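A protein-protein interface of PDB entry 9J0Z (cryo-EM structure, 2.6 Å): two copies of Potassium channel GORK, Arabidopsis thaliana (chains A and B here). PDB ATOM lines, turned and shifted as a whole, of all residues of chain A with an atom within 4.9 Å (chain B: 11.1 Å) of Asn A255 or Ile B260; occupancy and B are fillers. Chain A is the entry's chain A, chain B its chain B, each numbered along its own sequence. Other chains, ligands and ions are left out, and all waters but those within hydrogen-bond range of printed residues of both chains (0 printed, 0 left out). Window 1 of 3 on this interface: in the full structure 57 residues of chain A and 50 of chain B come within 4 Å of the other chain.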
ATOM      1  N   ARG A 150     -13.554  -8.449  11.531  1.00  0.00           N
ATOM      2  CA  ARG A 150     -14.270  -8.463  10.260  1.00  0.00           C
ATOM      3  C   ARG A 150     -13.418  -8.001   9.096  1.00  0.00           C
ATOM      4  O   ARG A 150     -13.419  -8.646   8.048  1.00  0.00           O
ATOM      5  CB  ARG A 150     -15.531  -7.616  10.345  1.00  0.00           C
ATOM      6  CG  ARG A 150     -16.339  -7.571   9.066  1.00  0.00           C
ATOM      7  CD  ARG A 150     -16.690  -8.961   8.579  1.00  0.00           C
ATOM      8  NE  ARG A 150     -15.849  -9.362   7.461  1.00  0.00           N
ATOM      9  CZ  ARG A 150     -16.032 -10.475   6.772  1.00  0.00           C
ATOM     10  NH1 ARG A 150     -17.026 -11.288   7.093  1.00  0.00           N
ATOM     11  NH2 ARG A 150     -15.231 -10.776   5.765  1.00  0.00           N
ATOM     12  N   ILE A 151     -12.722  -6.883   9.242  1.00  0.00           N
ATOM     13  CA  ILE A 151     -11.653  -6.519   8.327  1.00  0.00           C
ATOM     14  C   ILE A 151     -10.345  -7.179   8.705  1.00  0.00           C
ATOM     15  O   ILE A 151      -9.400  -7.144   7.907  1.00  0.00           O
ATOM     16  CB  ILE A 151     -11.475  -4.992   8.259  1.00  0.00           C
ATOM     17  CG1 ILE A 151     -10.725  -4.503   9.496  1.00  0.00           C
ATOM     18  CG2 ILE A 151     -12.826  -4.332   8.207  1.00  0.00           C
ATOM     19  CD1 ILE A 151     -10.117  -3.121   9.374  1.00  0.00           C
ATOM     20  N   LEU A 154      -9.302  -9.670   6.613  1.00  0.00           N
ATOM     21  CA  LEU A 154      -8.882  -9.151   5.327  1.00  0.00           C
ATOM     22  C   LEU A 154      -7.552  -8.440   5.437  1.00  0.00           C
ATOM     23  O   LEU A 154      -6.930  -8.160   4.416  1.00  0.00           O
ATOM     24  CB  LEU A 154      -9.935  -8.205   4.753  1.00  0.00           C
ATOM     25  CG  LEU A 154     -11.169  -8.915   4.240  1.00  0.00           C
ATOM     26  CD1 LEU A 154     -12.255  -7.922   4.061  1.00  0.00           C
ATOM     27  CD2 LEU A 154     -10.838  -9.531   2.922  1.00  0.00           C
ATOM     28  N   TYR A 251     -13.016  -5.121  -1.920  1.00  0.00           N
ATOM     29  CA  TYR A 251     -13.633  -5.837  -0.823  1.00  0.00           C
ATOM     30  C   TYR A 251     -13.250  -5.263   0.526  1.00  0.00           C
ATOM     31  O   TYR A 251     -14.089  -5.200   1.420  1.00  0.00           O
ATOM     32  CB  TYR A 251     -13.234  -7.301  -0.897  1.00  0.00           C
ATOM     33  CG  TYR A 251     -14.166  -8.233  -0.209  1.00  0.00           C
ATOM     34  CD1 TYR A 251     -15.416  -8.502  -0.730  1.00  0.00           C
ATOM     35  CD2 TYR A 251     -13.788  -8.865   0.956  1.00  0.00           C
ATOM     36  CE1 TYR A 251     -16.273  -9.365  -0.092  1.00  0.00           C
ATOM     37  CE2 TYR A 251     -14.628  -9.725   1.603  1.00  0.00           C
ATOM     38  CZ  TYR A 251     -15.871  -9.974   1.079  1.00  0.00           C
ATOM     39  OH  TYR A 251     -16.714 -10.843   1.732  1.00  0.00           O
ATOM     40  N   LEU A 252     -12.022  -4.788   0.676  1.00  0.00           N
ATOM     41  CA  LEU A 252     -11.616  -4.136   1.912  1.00  0.00           C
ATOM     42  C   LEU A 252     -12.308  -2.794   2.082  1.00  0.00           C
ATOM     43  O   LEU A 252     -12.766  -2.458   3.175  1.00  0.00           O
ATOM     44  CB  LEU A 252     -10.108  -3.961   1.928  1.00  0.00           C
ATOM     45  CG  LEU A 252      -9.571  -3.192   3.114  1.00  0.00           C
ATOM     46  CD1 LEU A 252      -9.416  -4.139   4.255  1.00  0.00           C
ATOM     47  CD2 LEU A 252      -8.263  -2.533   2.791  1.00  0.00           C
ATOM     48  N   ILE A 253     -12.397  -2.010   1.008  1.00  0.00           N
ATOM     49  CA  ILE A 253     -13.113  -0.739   1.069  1.00  0.00           C
ATOM     50  C   ILE A 253     -14.586  -0.971   1.347  1.00  0.00           C
ATOM     51  O   ILE A 253     -15.199  -0.251   2.138  1.00  0.00           O
ATOM     52  CB  ILE A 253     -12.899   0.060  -0.225  1.00  0.00           C
ATOM     53  CG1 ILE A 253     -11.438   0.426  -0.381  1.00  0.00           C
ATOM     54  CG2 ILE A 253     -13.672   1.328  -0.203  1.00  0.00           C
ATOM     55  CD1 ILE A 253     -11.133   1.060  -1.679  1.00  0.00           C
ATOM     56  N   GLY A 254     -15.159  -2.024   0.767  1.00  0.00           N
ATOM     57  CA  GLY A 254     -16.549  -2.345   1.033  1.00  0.00           C
ATOM     58  C   GLY A 254     -16.801  -2.787   2.458  1.00  0.00           C
ATOM     59  O   GLY A 254     -17.808  -2.415   3.055  1.00  0.00           O
ATOM     60  N   ASN A 255     -15.880  -3.551   3.032  1.00  0.00           N
ATOM     61  CA  ASN A 255     -16.035  -3.975   4.416  1.00  0.00           C
ATOM     62  C   ASN A 255     -15.891  -2.814   5.380  1.00  0.00           C
ATOM     63  O   ASN A 255     -16.687  -2.680   6.312  1.00  0.00           O
ATOM     64  CB  ASN A 255     -15.018  -5.042   4.746  1.00  0.00           C
ATOM     65  CG  ASN A 255     -15.571  -6.399   4.602  1.00  0.00           C
ATOM     66  OD1 ASN A 255     -16.105  -6.957   5.544  1.00  0.00           O
ATOM     67  ND2 ASN A 255     -15.476  -6.947   3.414  1.00  0.00           N
ATOM     68  N   ILE A 256     -14.887  -1.964   5.171  1.00  0.00           N
ATOM     69  CA  ILE A 256     -14.690  -0.824   6.054  1.00  0.00           C
ATOM     70  C   ILE A 256     -15.817   0.186   5.887  1.00  0.00           C
ATOM     71  O   ILE A 256     -16.197   0.863   6.843  1.00  0.00           O
ATOM     72  CB  ILE A 256     -13.302  -0.219   5.800  1.00  0.00           C
ATOM     73  CG1 ILE A 256     -12.239  -1.234   6.148  1.00  0.00           C
ATOM     74  CG2 ILE A 256     -13.044   0.946   6.673  1.00  0.00           C
ATOM     75  CD1 ILE A 256     -10.863  -0.786   5.855  1.00  0.00           C
ATOM     76  N   THR A 257     -16.428   0.254   4.712  1.00  0.00           N
ATOM     77  CA  THR A 257     -17.581   1.120   4.554  1.00  0.00           C
ATOM     78  C   THR A 257     -18.807   0.571   5.259  1.00  0.00           C
ATOM     79  O   THR A 257     -19.421   1.276   6.061  1.00  0.00           O
ATOM     80  CB  THR A 257     -17.891   1.310   3.093  1.00  0.00           C
ATOM     81  OG1 THR A 257     -16.794   1.966   2.464  1.00  0.00           O
ATOM     82  CG2 THR A 257     -19.061   2.156   2.973  1.00  0.00           C
ATOM     83  N   ALA A 258     -19.163  -0.685   5.007  1.00  0.00           N
ATOM     84  CA  ALA A 258     -20.335  -1.301   5.607  1.00  0.00           C
ATOM     85  C   ALA A 258     -20.199  -1.513   7.104  1.00  0.00           C
ATOM     86  O   ALA A 258     -21.199  -1.752   7.776  1.00  0.00           O
ATOM     87  CB  ALA A 258     -20.630  -2.630   4.931  1.00  0.00           C
ATOM     88  N   LEU A 259     -18.996  -1.427   7.646  1.00  0.00           N
ATOM     89  CA  LEU A 259     -18.814  -1.384   9.085  1.00  0.00           C
ATOM     90  C   LEU A 259     -19.003   0.021   9.632  1.00  0.00           C
ATOM     91  O   LEU A 259     -19.142   0.187  10.842  1.00  0.00           O
ATOM     92  CB  LEU A 259     -17.426  -1.926   9.433  1.00  0.00           C
ATOM     93  CG  LEU A 259     -16.854  -2.132  10.828  1.00  0.00           C
ATOM     94  CD1 LEU A 259     -15.969  -3.343  10.795  1.00  0.00           C
ATOM     95  CD2 LEU A 259     -16.030  -0.933  11.242  1.00  0.00           C
ATOM     96  N   LYS A 262     -23.182   1.053   9.145  1.00  0.00           N
ATOM     97  CA  LYS A 262     -23.933   0.483  10.251  1.00  0.00           C
ATOM     98  C   LYS A 262     -23.395   1.039  11.556  1.00  0.00           C
ATOM     99  O   LYS A 262     -22.910   0.287  12.407  1.00  0.00           O
ATOM    100  CB  LYS A 262     -23.858  -1.040  10.247  1.00  0.00           C
ATOM    101  CG  LYS A 262     -24.255  -1.654   8.933  1.00  0.00           C
ATOM    102  CD  LYS A 262     -24.171  -3.162   8.985  1.00  0.00           C
ATOM    103  CE  LYS A 262     -24.431  -3.766   7.619  1.00  0.00           C
ATOM    104  NZ  LYS A 262     -25.713  -4.512   7.597  1.00  0.00           N
ATOM    105  N   ASN B 145     -27.327 -14.436  -5.890  1.00  0.00           N
ATOM    106  CA  ASN B 145     -27.730 -13.054  -5.662  1.00  0.00           C
ATOM    107  C   ASN B 145     -27.780 -12.293  -6.978  1.00  0.00           C
ATOM    108  O   ASN B 145     -26.958 -12.510  -7.867  1.00  0.00           O
ATOM    109  CB  ASN B 145     -26.741 -12.392  -4.700  1.00  0.00           C
ATOM    110  CG  ASN B 145     -27.282 -11.123  -4.067  1.00  0.00           C
ATOM    111  OD1 ASN B 145     -27.846 -10.259  -4.733  1.00  0.00           O
ATOM    112  ND2 ASN B 145     -27.106 -11.008  -2.759  1.00  0.00           N
ATOM    113  N   TYR B 146     -28.759 -11.405  -7.109  1.00  0.00           N
ATOM    114  CA  TYR B 146     -28.800 -10.566  -8.297  1.00  0.00           C
ATOM    115  C   TYR B 146     -27.714  -9.520  -8.291  1.00  0.00           C
ATOM    116  O   TYR B 146     -27.329  -9.047  -9.362  1.00  0.00           O
ATOM    117  CB  TYR B 146     -30.153  -9.869  -8.446  1.00  0.00           C
ATOM    118  CG  TYR B 146     -30.322  -8.627  -7.598  1.00  0.00           C
ATOM    119  CD1 TYR B 146     -30.599  -8.729  -6.243  1.00  0.00           C
ATOM    120  CD2 TYR B 146     -30.225  -7.355  -8.155  1.00  0.00           C
ATOM    121  CE1 TYR B 146     -30.761  -7.610  -5.464  1.00  0.00           C
ATOM    122  CE2 TYR B 146     -30.375  -6.230  -7.379  1.00  0.00           C
ATOM    123  CZ  TYR B 146     -30.650  -6.362  -6.036  1.00  0.00           C
ATOM    124  OH  TYR B 146     -30.812  -5.241  -5.257  1.00  0.00           O
ATOM    125  N   LEU B 147     -27.235  -9.129  -7.121  1.00  0.00           N
ATOM    126  CA  LEU B 147     -26.229  -8.090  -7.049  1.00  0.00           C
ATOM    127  C   LEU B 147     -24.830  -8.677  -7.125  1.00  0.00           C
ATOM    128  O   LEU B 147     -23.876  -7.951  -7.411  1.00  0.00           O
ATOM    129  CB  LEU B 147     -26.447  -7.275  -5.775  1.00  0.00           C
ATOM    130  CG  LEU B 147     -25.971  -5.831  -5.751  1.00  0.00           C
ATOM    131  CD1 LEU B 147     -26.931  -5.018  -4.924  1.00  0.00           C
ATOM    132  CD2 LEU B 147     -24.630  -5.740  -5.147  1.00  0.00           C
ATOM    133  N   PHE B 148     -24.707  -9.987  -6.925  1.00  0.00           N
ATOM    134  CA  PHE B 148     -23.466 -10.681  -7.230  1.00  0.00           C
ATOM    135  C   PHE B 148     -23.229 -10.741  -8.730  1.00  0.00           C
ATOM    136  O   PHE B 148     -22.088 -10.612  -9.187  1.00  0.00           O
ATOM    137  CB  PHE B 148     -23.520 -12.078  -6.630  1.00  0.00           C
ATOM    138  CG  PHE B 148     -22.235 -12.821  -6.692  1.00  0.00           C
ATOM    139  CD1 PHE B 148     -22.126 -13.958  -7.463  1.00  0.00           C
ATOM    140  CD2 PHE B 148     -21.148 -12.408  -5.958  1.00  0.00           C
ATOM    141  CE1 PHE B 148     -20.951 -14.661  -7.514  1.00  0.00           C
ATOM    142  CE2 PHE B 148     -19.969 -13.106  -6.007  1.00  0.00           C
ATOM    143  CZ  PHE B 148     -19.870 -14.235  -6.787  1.00  0.00           C
ATOM    144  N   ARG B 150     -24.384  -8.409 -10.634  1.00  0.00           N
ATOM    145  CA  ARG B 150     -24.021  -7.040 -10.962  1.00  0.00           C
ATOM    146  C   ARG B 150     -22.581  -6.720 -10.605  1.00  0.00           C
ATOM    147  O   ARG B 150     -22.123  -5.617 -10.892  1.00  0.00           O
ATOM    148  CB  ARG B 150     -24.959  -6.057 -10.270  1.00  0.00           C
ATOM    149  CG  ARG B 150     -26.216  -5.783 -11.065  1.00  0.00           C
ATOM    150  CD  ARG B 150     -27.264  -5.023 -10.270  1.00  0.00           C
ATOM    151  NE  ARG B 150     -26.819  -3.694  -9.871  1.00  0.00           N
ATOM    152  CZ  ARG B 150     -26.939  -2.608 -10.625  1.00  0.00           C
ATOM    153  NH1 ARG B 150     -27.483  -2.687 -11.829  1.00  0.00           N
ATOM    154  NH2 ARG B 150     -26.508  -1.442 -10.177  1.00  0.00           N
ATOM    155  N   ILE B 151     -21.868  -7.643  -9.965  1.00  0.00           N
ATOM    156  CA  ILE B 151     -20.426  -7.524  -9.817  1.00  0.00           C
ATOM    157  C   ILE B 151     -19.721  -8.305 -10.912  1.00  0.00           C
ATOM    158  O   ILE B 151     -18.767  -7.818 -11.523  1.00  0.00           O
ATOM    159  CB  ILE B 151     -20.014  -8.004  -8.418  1.00  0.00           C
ATOM    160  CG1 ILE B 151     -20.509  -7.028  -7.369  1.00  0.00           C
ATOM    161  CG2 ILE B 151     -18.521  -8.168  -8.305  1.00  0.00           C
ATOM    162  CD1 ILE B 151     -20.668  -7.654  -6.032  1.00  0.00           C
ATOM    163  N   TYR B 251     -17.460   2.238  -9.721  1.00  0.00           N
ATOM    164  CA  TYR B 251     -18.682   1.483  -9.870  1.00  0.00           C
ATOM    165  C   TYR B 251     -18.545   0.064  -9.348  1.00  0.00           C
ATOM    166  O   TYR B 251     -19.484  -0.455  -8.747  1.00  0.00           O
ATOM    167  CB  TYR B 251     -19.043   1.494 -11.337  1.00  0.00           C
ATOM    168  CG  TYR B 251     -20.475   1.268 -11.601  1.00  0.00           C
ATOM    169  CD1 TYR B 251     -21.391   2.263 -11.342  1.00  0.00           C
ATOM    170  CD2 TYR B 251     -20.918   0.086 -12.144  1.00  0.00           C
ATOM    171  CE1 TYR B 251     -22.713   2.078 -11.590  1.00  0.00           C
ATOM    172  CE2 TYR B 251     -22.243  -0.114 -12.400  1.00  0.00           C
ATOM    173  CZ  TYR B 251     -23.138   0.886 -12.118  1.00  0.00           C
ATOM    174  OH  TYR B 251     -24.474   0.688 -12.375  1.00  0.00           O
ATOM    175  N   LEU B 252     -17.390  -0.558  -9.526  1.00  0.00           N
ATOM    176  CA  LEU B 252     -17.052  -1.837  -8.921  1.00  0.00           C
ATOM    177  C   LEU B 252     -17.044  -1.789  -7.402  1.00  0.00           C
ATOM    178  O   LEU B 252     -17.646  -2.651  -6.754  1.00  0.00           O
ATOM    179  CB  LEU B 252     -15.680  -2.286  -9.400  1.00  0.00           C
ATOM    180  CG  LEU B 252     -15.186  -3.599  -8.824  1.00  0.00           C
ATOM    181  CD1 LEU B 252     -15.921  -4.734  -9.463  1.00  0.00           C
ATOM    182  CD2 LEU B 252     -13.713  -3.749  -9.014  1.00  0.00           C
ATOM    183  N   ILE B 253     -16.349  -0.808  -6.827  1.00  0.00           N
ATOM    184  CA  ILE B 253     -16.336  -0.604  -5.385  1.00  0.00           C
ATOM    185  C   ILE B 253     -17.722  -0.302  -4.861  1.00  0.00           C
ATOM    186  O   ILE B 253     -18.097  -0.806  -3.799  1.00  0.00           O
ATOM    187  CB  ILE B 253     -15.355   0.523  -5.037  1.00  0.00           C
ATOM    188  CG1 ILE B 253     -13.943   0.098  -5.367  1.00  0.00           C
ATOM    189  CG2 ILE B 253     -15.392   0.873  -3.591  1.00  0.00           C
ATOM    190  CD1 ILE B 253     -12.987   1.218  -5.380  1.00  0.00           C
ATOM    191  N   GLY B 254     -18.508   0.451  -5.611  1.00  0.00           N
ATOM    192  CA  GLY B 254     -19.884   0.705  -5.280  1.00  0.00           C
ATOM    193  C   GLY B 254     -20.738  -0.530  -5.204  1.00  0.00           C
ATOM    194  O   GLY B 254     -21.482  -0.709  -4.247  1.00  0.00           O
ATOM    195  N   ASN B 255     -20.612  -1.410  -6.180  1.00  0.00           N
ATOM    196  CA  ASN B 255     -21.403  -2.624  -6.155  1.00  0.00           C
ATOM    197  C   ASN B 255     -20.956  -3.599  -5.090  1.00  0.00           C
ATOM    198  O   ASN B 255     -21.802  -4.254  -4.485  1.00  0.00           O
ATOM    199  CB  ASN B 255     -21.364  -3.290  -7.510  1.00  0.00           C
ATOM    200  CG  ASN B 255     -22.385  -2.734  -8.419  1.00  0.00           C
ATOM    201  OD1 ASN B 255     -22.071  -2.190  -9.457  1.00  0.00           O
ATOM    202  ND2 ASN B 255     -23.631  -2.830  -8.022  1.00  0.00           N
ATOM    203  N   ILE B 256     -19.663  -3.689  -4.816  1.00  0.00           N
ATOM    204  CA  ILE B 256     -19.198  -4.569  -3.753  1.00  0.00           C
ATOM    205  C   ILE B 256     -19.653  -4.060  -2.393  1.00  0.00           C
ATOM    206  O   ILE B 256     -20.118  -4.832  -1.548  1.00  0.00           O
ATOM    207  CB  ILE B 256     -17.676  -4.722  -3.848  1.00  0.00           C
ATOM    208  CG1 ILE B 256     -17.368  -5.569  -5.066  1.00  0.00           C
ATOM    209  CG2 ILE B 256     -17.130  -5.348  -2.629  1.00  0.00           C
ATOM    210  CD1 ILE B 256     -15.954  -5.954  -5.211  1.00  0.00           C
ATOM    211  N   THR B 257     -19.608  -2.745  -2.193  1.00  0.00           N
ATOM    212  CA  THR B 257     -20.107  -2.153  -0.960  1.00  0.00           C
ATOM    213  C   THR B 257     -21.605  -2.355  -0.813  1.00  0.00           C
ATOM    214  O   THR B 257     -22.092  -2.677   0.273  1.00  0.00           O
ATOM    215  CB  THR B 257     -19.771  -0.673  -0.938  1.00  0.00           C
ATOM    216  OG1 THR B 257     -18.361  -0.509  -1.054  1.00  0.00           O
ATOM    217  CG2 THR B 257     -20.222  -0.058   0.322  1.00  0.00           C
ATOM    218  N   ALA B 258     -22.352  -2.215  -1.905  1.00  0.00           N
ATOM    219  CA  ALA B 258     -23.794  -2.401  -1.836  1.00  0.00           C
ATOM    220  C   ALA B 258     -24.156  -3.856  -1.598  1.00  0.00           C
ATOM    221  O   ALA B 258     -25.226  -4.159  -1.074  1.00  0.00           O
ATOM    222  CB  ALA B 258     -24.450  -1.886  -3.109  1.00  0.00           C
ATOM    223  N   LEU B 259     -23.281  -4.774  -1.986  1.00  0.00           N
ATOM    224  CA  LEU B 259     -23.479  -6.167  -1.612  1.00  0.00           C
ATOM    225  C   LEU B 259     -23.233  -6.375  -0.131  1.00  0.00           C
ATOM    226  O   LEU B 259     -23.956  -7.119   0.530  1.00  0.00           O
ATOM    227  CB  LEU B 259     -22.551  -7.063  -2.418  1.00  0.00           C
ATOM    228  CG  LEU B 259     -22.763  -8.559  -2.282  1.00  0.00           C
ATOM    229  CD1 LEU B 259     -23.957  -8.955  -3.089  1.00  0.00           C
ATOM    230  CD2 LEU B 259     -21.541  -9.290  -2.766  1.00  0.00           C
ATOM    231  N   ILE B 260     -22.207  -5.730   0.409  1.00  0.00           N
ATOM    232  CA  ILE B 260     -21.793  -6.017   1.779  1.00  0.00           C
ATOM    233  C   ILE B 260     -22.711  -5.333   2.792  1.00  0.00           C
ATOM    234  O   ILE B 260     -22.959  -5.882   3.869  1.00  0.00           O
ATOM    235  CB  ILE B 260     -20.310  -5.654   1.972  1.00  0.00           C
ATOM    236  CG1 ILE B 260     -19.469  -6.574   1.107  1.00  0.00           C
ATOM    237  CG2 ILE B 260     -19.846  -5.912   3.362  1.00  0.00           C
ATOM    238  CD1 ILE B 260     -18.006  -6.305   1.147  1.00  0.00           C
ATOM    239  N   VAL B 261     -23.307  -4.191   2.448  1.00  0.00           N
ATOM    240  CA  VAL B 261     -24.253  -3.544   3.359  1.00  0.00           C
ATOM    241  C   VAL B 261     -25.538  -4.328   3.549  1.00  0.00           C
ATOM    242  O   VAL B 261     -26.266  -4.054   4.513  1.00  0.00           O
ATOM    243  CB  VAL B 261     -24.606  -2.106   2.929  1.00  0.00           C
ATOM    244  CG1 VAL B 261     -23.395  -1.232   2.908  1.00  0.00           C
ATOM    245  CG2 VAL B 261     -25.300  -2.117   1.617  1.00  0.00           C
ATOM    246  N   LYS B 262     -25.854  -5.277   2.677  1.00  0.00           N
ATOM    247  CA  LYS B 262     -26.886  -6.265   2.961  1.00  0.00           C
ATOM    248  C   LYS B 262     -26.211  -7.502   3.546  1.00  0.00           C
ATOM    249  O   LYS B 262     -26.049  -8.533   2.901  1.00  0.00           O
ATOM    250  CB  LYS B 262     -27.671  -6.582   1.700  1.00  0.00           C
ATOM    251  CG  LYS B 262     -27.997  -5.360   0.895  1.00  0.00           C
ATOM    252  CD  LYS B 262     -28.974  -5.677  -0.213  1.00  0.00           C
ATOM    253  CE  LYS B 262     -30.350  -5.114   0.089  1.00  0.00           C
ATOM    254  NZ  LYS B 262     -31.204  -5.051  -1.126  1.00  0.00           N
ATOM    255  N   GLY B 263     -25.815  -7.359   4.806  1.00  0.00           N
ATOM    256  CA  GLY B 263     -24.782  -8.183   5.402  1.00  0.00           C
ATOM    257  C   GLY B 263     -25.073  -9.650   5.625  1.00  0.00           C
ATOM    258  O   GLY B 263     -26.133 -10.159   5.248  1.00  0.00           O
ATOM    259  N   SER B 264     -24.127 -10.334   6.262  1.00  0.00           N
ATOM    260  CA  SER B 264     -24.152 -11.780   6.388  1.00  0.00           C
ATOM    261  C   SER B 264     -24.850 -12.212   7.668  1.00  0.00           C
ATOM    262  O   SER B 264     -25.228 -11.392   8.505  1.00  0.00           O
ATOM    263  CB  SER B 264     -22.741 -12.357   6.367  1.00  0.00           C
ATOM    264  OG  SER B 264     -22.759 -13.726   6.732  1.00  0.00           O
ATOM    265  N   ASN B 265     -24.990 -13.528   7.818  1.00  0.00           N
ATOM    266  CA  ASN B 265     -25.804 -14.069   8.895  1.00  0.00           C
ATOM    267  C   ASN B 265     -25.078 -14.021  10.228  1.00  0.00           C
ATOM    268  O   ASN B 265     -25.711 -14.049  11.286  1.00  0.00           O
ATOM    269  CB  ASN B 265     -26.209 -15.498   8.560  1.00  0.00           C
ATOM    270  CG  ASN B 265     -27.518 -15.563   7.822  1.00  0.00           C
ATOM    271  OD1 ASN B 265     -28.346 -14.658   7.921  1.00  0.00           O
ATOM    272  ND2 ASN B 265     -27.717 -16.638   7.073  1.00  0.00           N
ATOM    273  N   THR B 266     -23.749 -13.939  10.205  1.00  0.00           N
ATOM    274  CA  THR B 266     -23.012 -13.837  11.458  1.00  0.00           C
ATOM    275  C   THR B 266     -23.109 -12.428  12.041  1.00  0.00           C
ATOM    276  O   THR B 266     -23.263 -12.253  13.257  1.00  0.00           O
ATOM    277  CB  THR B 266     -21.556 -14.293  11.264  1.00  0.00           C
ATOM    278  OG1 THR B 266     -20.859 -14.235  12.514  1.00  0.00           O
ATOM    279  CG2 THR B 266     -20.808 -13.504  10.185  1.00  0.00           C
ATOM    280  N   GLU B 267     -23.097 -11.404  11.186  1.00  0.00           N
ATOM    281  CA  GLU B 267     -23.249 -10.056  11.712  1.00  0.00           C
ATOM    282  C   GLU B 267     -24.719  -9.733  11.914  1.00  0.00           C
ATOM    283  O   GLU B 267     -25.061  -8.854  12.704  1.00  0.00           O
ATOM    284  CB  GLU B 267     -22.552  -9.037  10.809  1.00  0.00           C
ATOM    285  CG  GLU B 267     -23.172  -8.790   9.463  1.00  0.00           C
ATOM    286  CD  GLU B 267     -24.033  -7.557   9.469  1.00  0.00           C
ATOM    287  OE1 GLU B 267     -23.837  -6.724  10.373  1.00  0.00           O
ATOM    288  OE2 GLU B 267     -24.895  -7.416   8.581  1.00  0.00           O
ATOM    289  N   ARG B 268     -25.611 -10.492  11.275  1.00  0.00           N
ATOM    290  CA  ARG B 268     -27.023 -10.415  11.638  1.00  0.00           C
ATOM    291  C   ARG B 268     -27.285 -11.089  12.980  1.00  0.00           C
ATOM    292  O   ARG B 268     -28.143 -10.640  13.750  1.00  0.00           O
ATOM    293  CB  ARG B 268     -27.879 -11.039  10.539  1.00  0.00           C
ATOM    294  CG  ARG B 268     -28.140 -10.107   9.382  1.00  0.00           C
ATOM    295  CD  ARG B 268     -29.576 -10.199   8.924  1.00  0.00           C
ATOM    296  NE  ARG B 268     -29.767 -11.289   7.979  1.00  0.00           N
ATOM    297  CZ  ARG B 268     -29.911 -11.116   6.671  1.00  0.00           C
ATOM    298  NH1 ARG B 268     -29.898  -9.892   6.160  1.00  0.00           N
ATOM    299  NH2 ARG B 268     -30.078 -12.164   5.876  1.00  0.00           N
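Asn A255 touches one residue of chain B. Of chain A, only Tyr A251 (3.7 Å), Gly A254 (3.9 Å), Asn A255 (3.5 Å) and Ala A258 (3.7 Å) come within 4 Å of Ile B260. Ile A151 touches none of the printed residues of chain B. Of chain B, only Thr B257 and Ile B260 come within 4 Å of Gly A254. No residue of chain B comes within 4 Å of Ile A256. Of the printed residues of chain A, Gly B263 touches Lys A262 (3.99 Å). Of the printed residues of chain A, Ile B253 touches Ile A253. Printed residues of chain B within 4 Å of Ile A253: Ile B253 (3.8 Å). Of the printed residues of chain B, Lys A262 touches Val B261, Gly B263 and Glu B267. Thr B266 touches none of the printed residues of chain A. The nearest residue of chain B that does not touch Asn A255 is Thr B257 (5.7 Å). The nearest printed residue of chain B that does not touch Ile A253 is Thr B257 (4.5 Å).
Among the printed residues, pairs that only touch across the chains: Tyr A251 with Ile B256, Tyr A251 with Ile B260, Ile A253 with Ile B253, Gly A254 with Thr B257, Gly A254 with Ile B260, Asn A255 with Ile B260, Thr A257 with Thr B257, Ala A258 with Ile B260, Ala A258 with Val B261 and Lys A262 with Gly B263.
The guanidinium group (NE) of Arg A150 is in hydrogen-bond range of the side-chain amide oxygen (OD1) of Asn A255 (3.1 Å). The side-chain amide nitrogen of Asn A255 lies within hydrogen-bond range of the backbone carbonyl oxygen of Tyr A251 (3.0 Å). The side-chain hydroxyl (OG1) of Thr A257 lies within hydrogen-bond range of the backbone carbonyl oxygen (O) of Ile A253. OG1 of Thr B257 is in hydrogen-bond range of O of Ile B253 (2.8 Å).
Tyr A251 touches Ile B256, but with the chains exchanged Ile A256 does not touch Tyr B251 (14.7 Å). Ile A253 touches its own counterpart, Ile B253. Gly A254 touches Thr B257, but with the chains exchanged Thr A257 does not touch Gly B254 (8.1 Å). Thr B257 touches its own counterpart, Thr A257.
NZ of Lys A262 sits at hydrogen-bond distance from O of Val B261 (3.2 Å). OE2 of Glu B267 lies within salt-bridge range of NZ of Lys A262, 3.2 Å away.
Hydrophobic or aromatic side chains of chain A that line the printed part of chain B: Tyr A251, Ile A253 and Ala A258. Among the printed residues, 12 pairs touch across the chains. Among the printed residues, Asp or Glu carboxylates within 4 Å of a Lys or Arg side-chain nitrogen of the other chain: Lys A262 with Glu B267.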
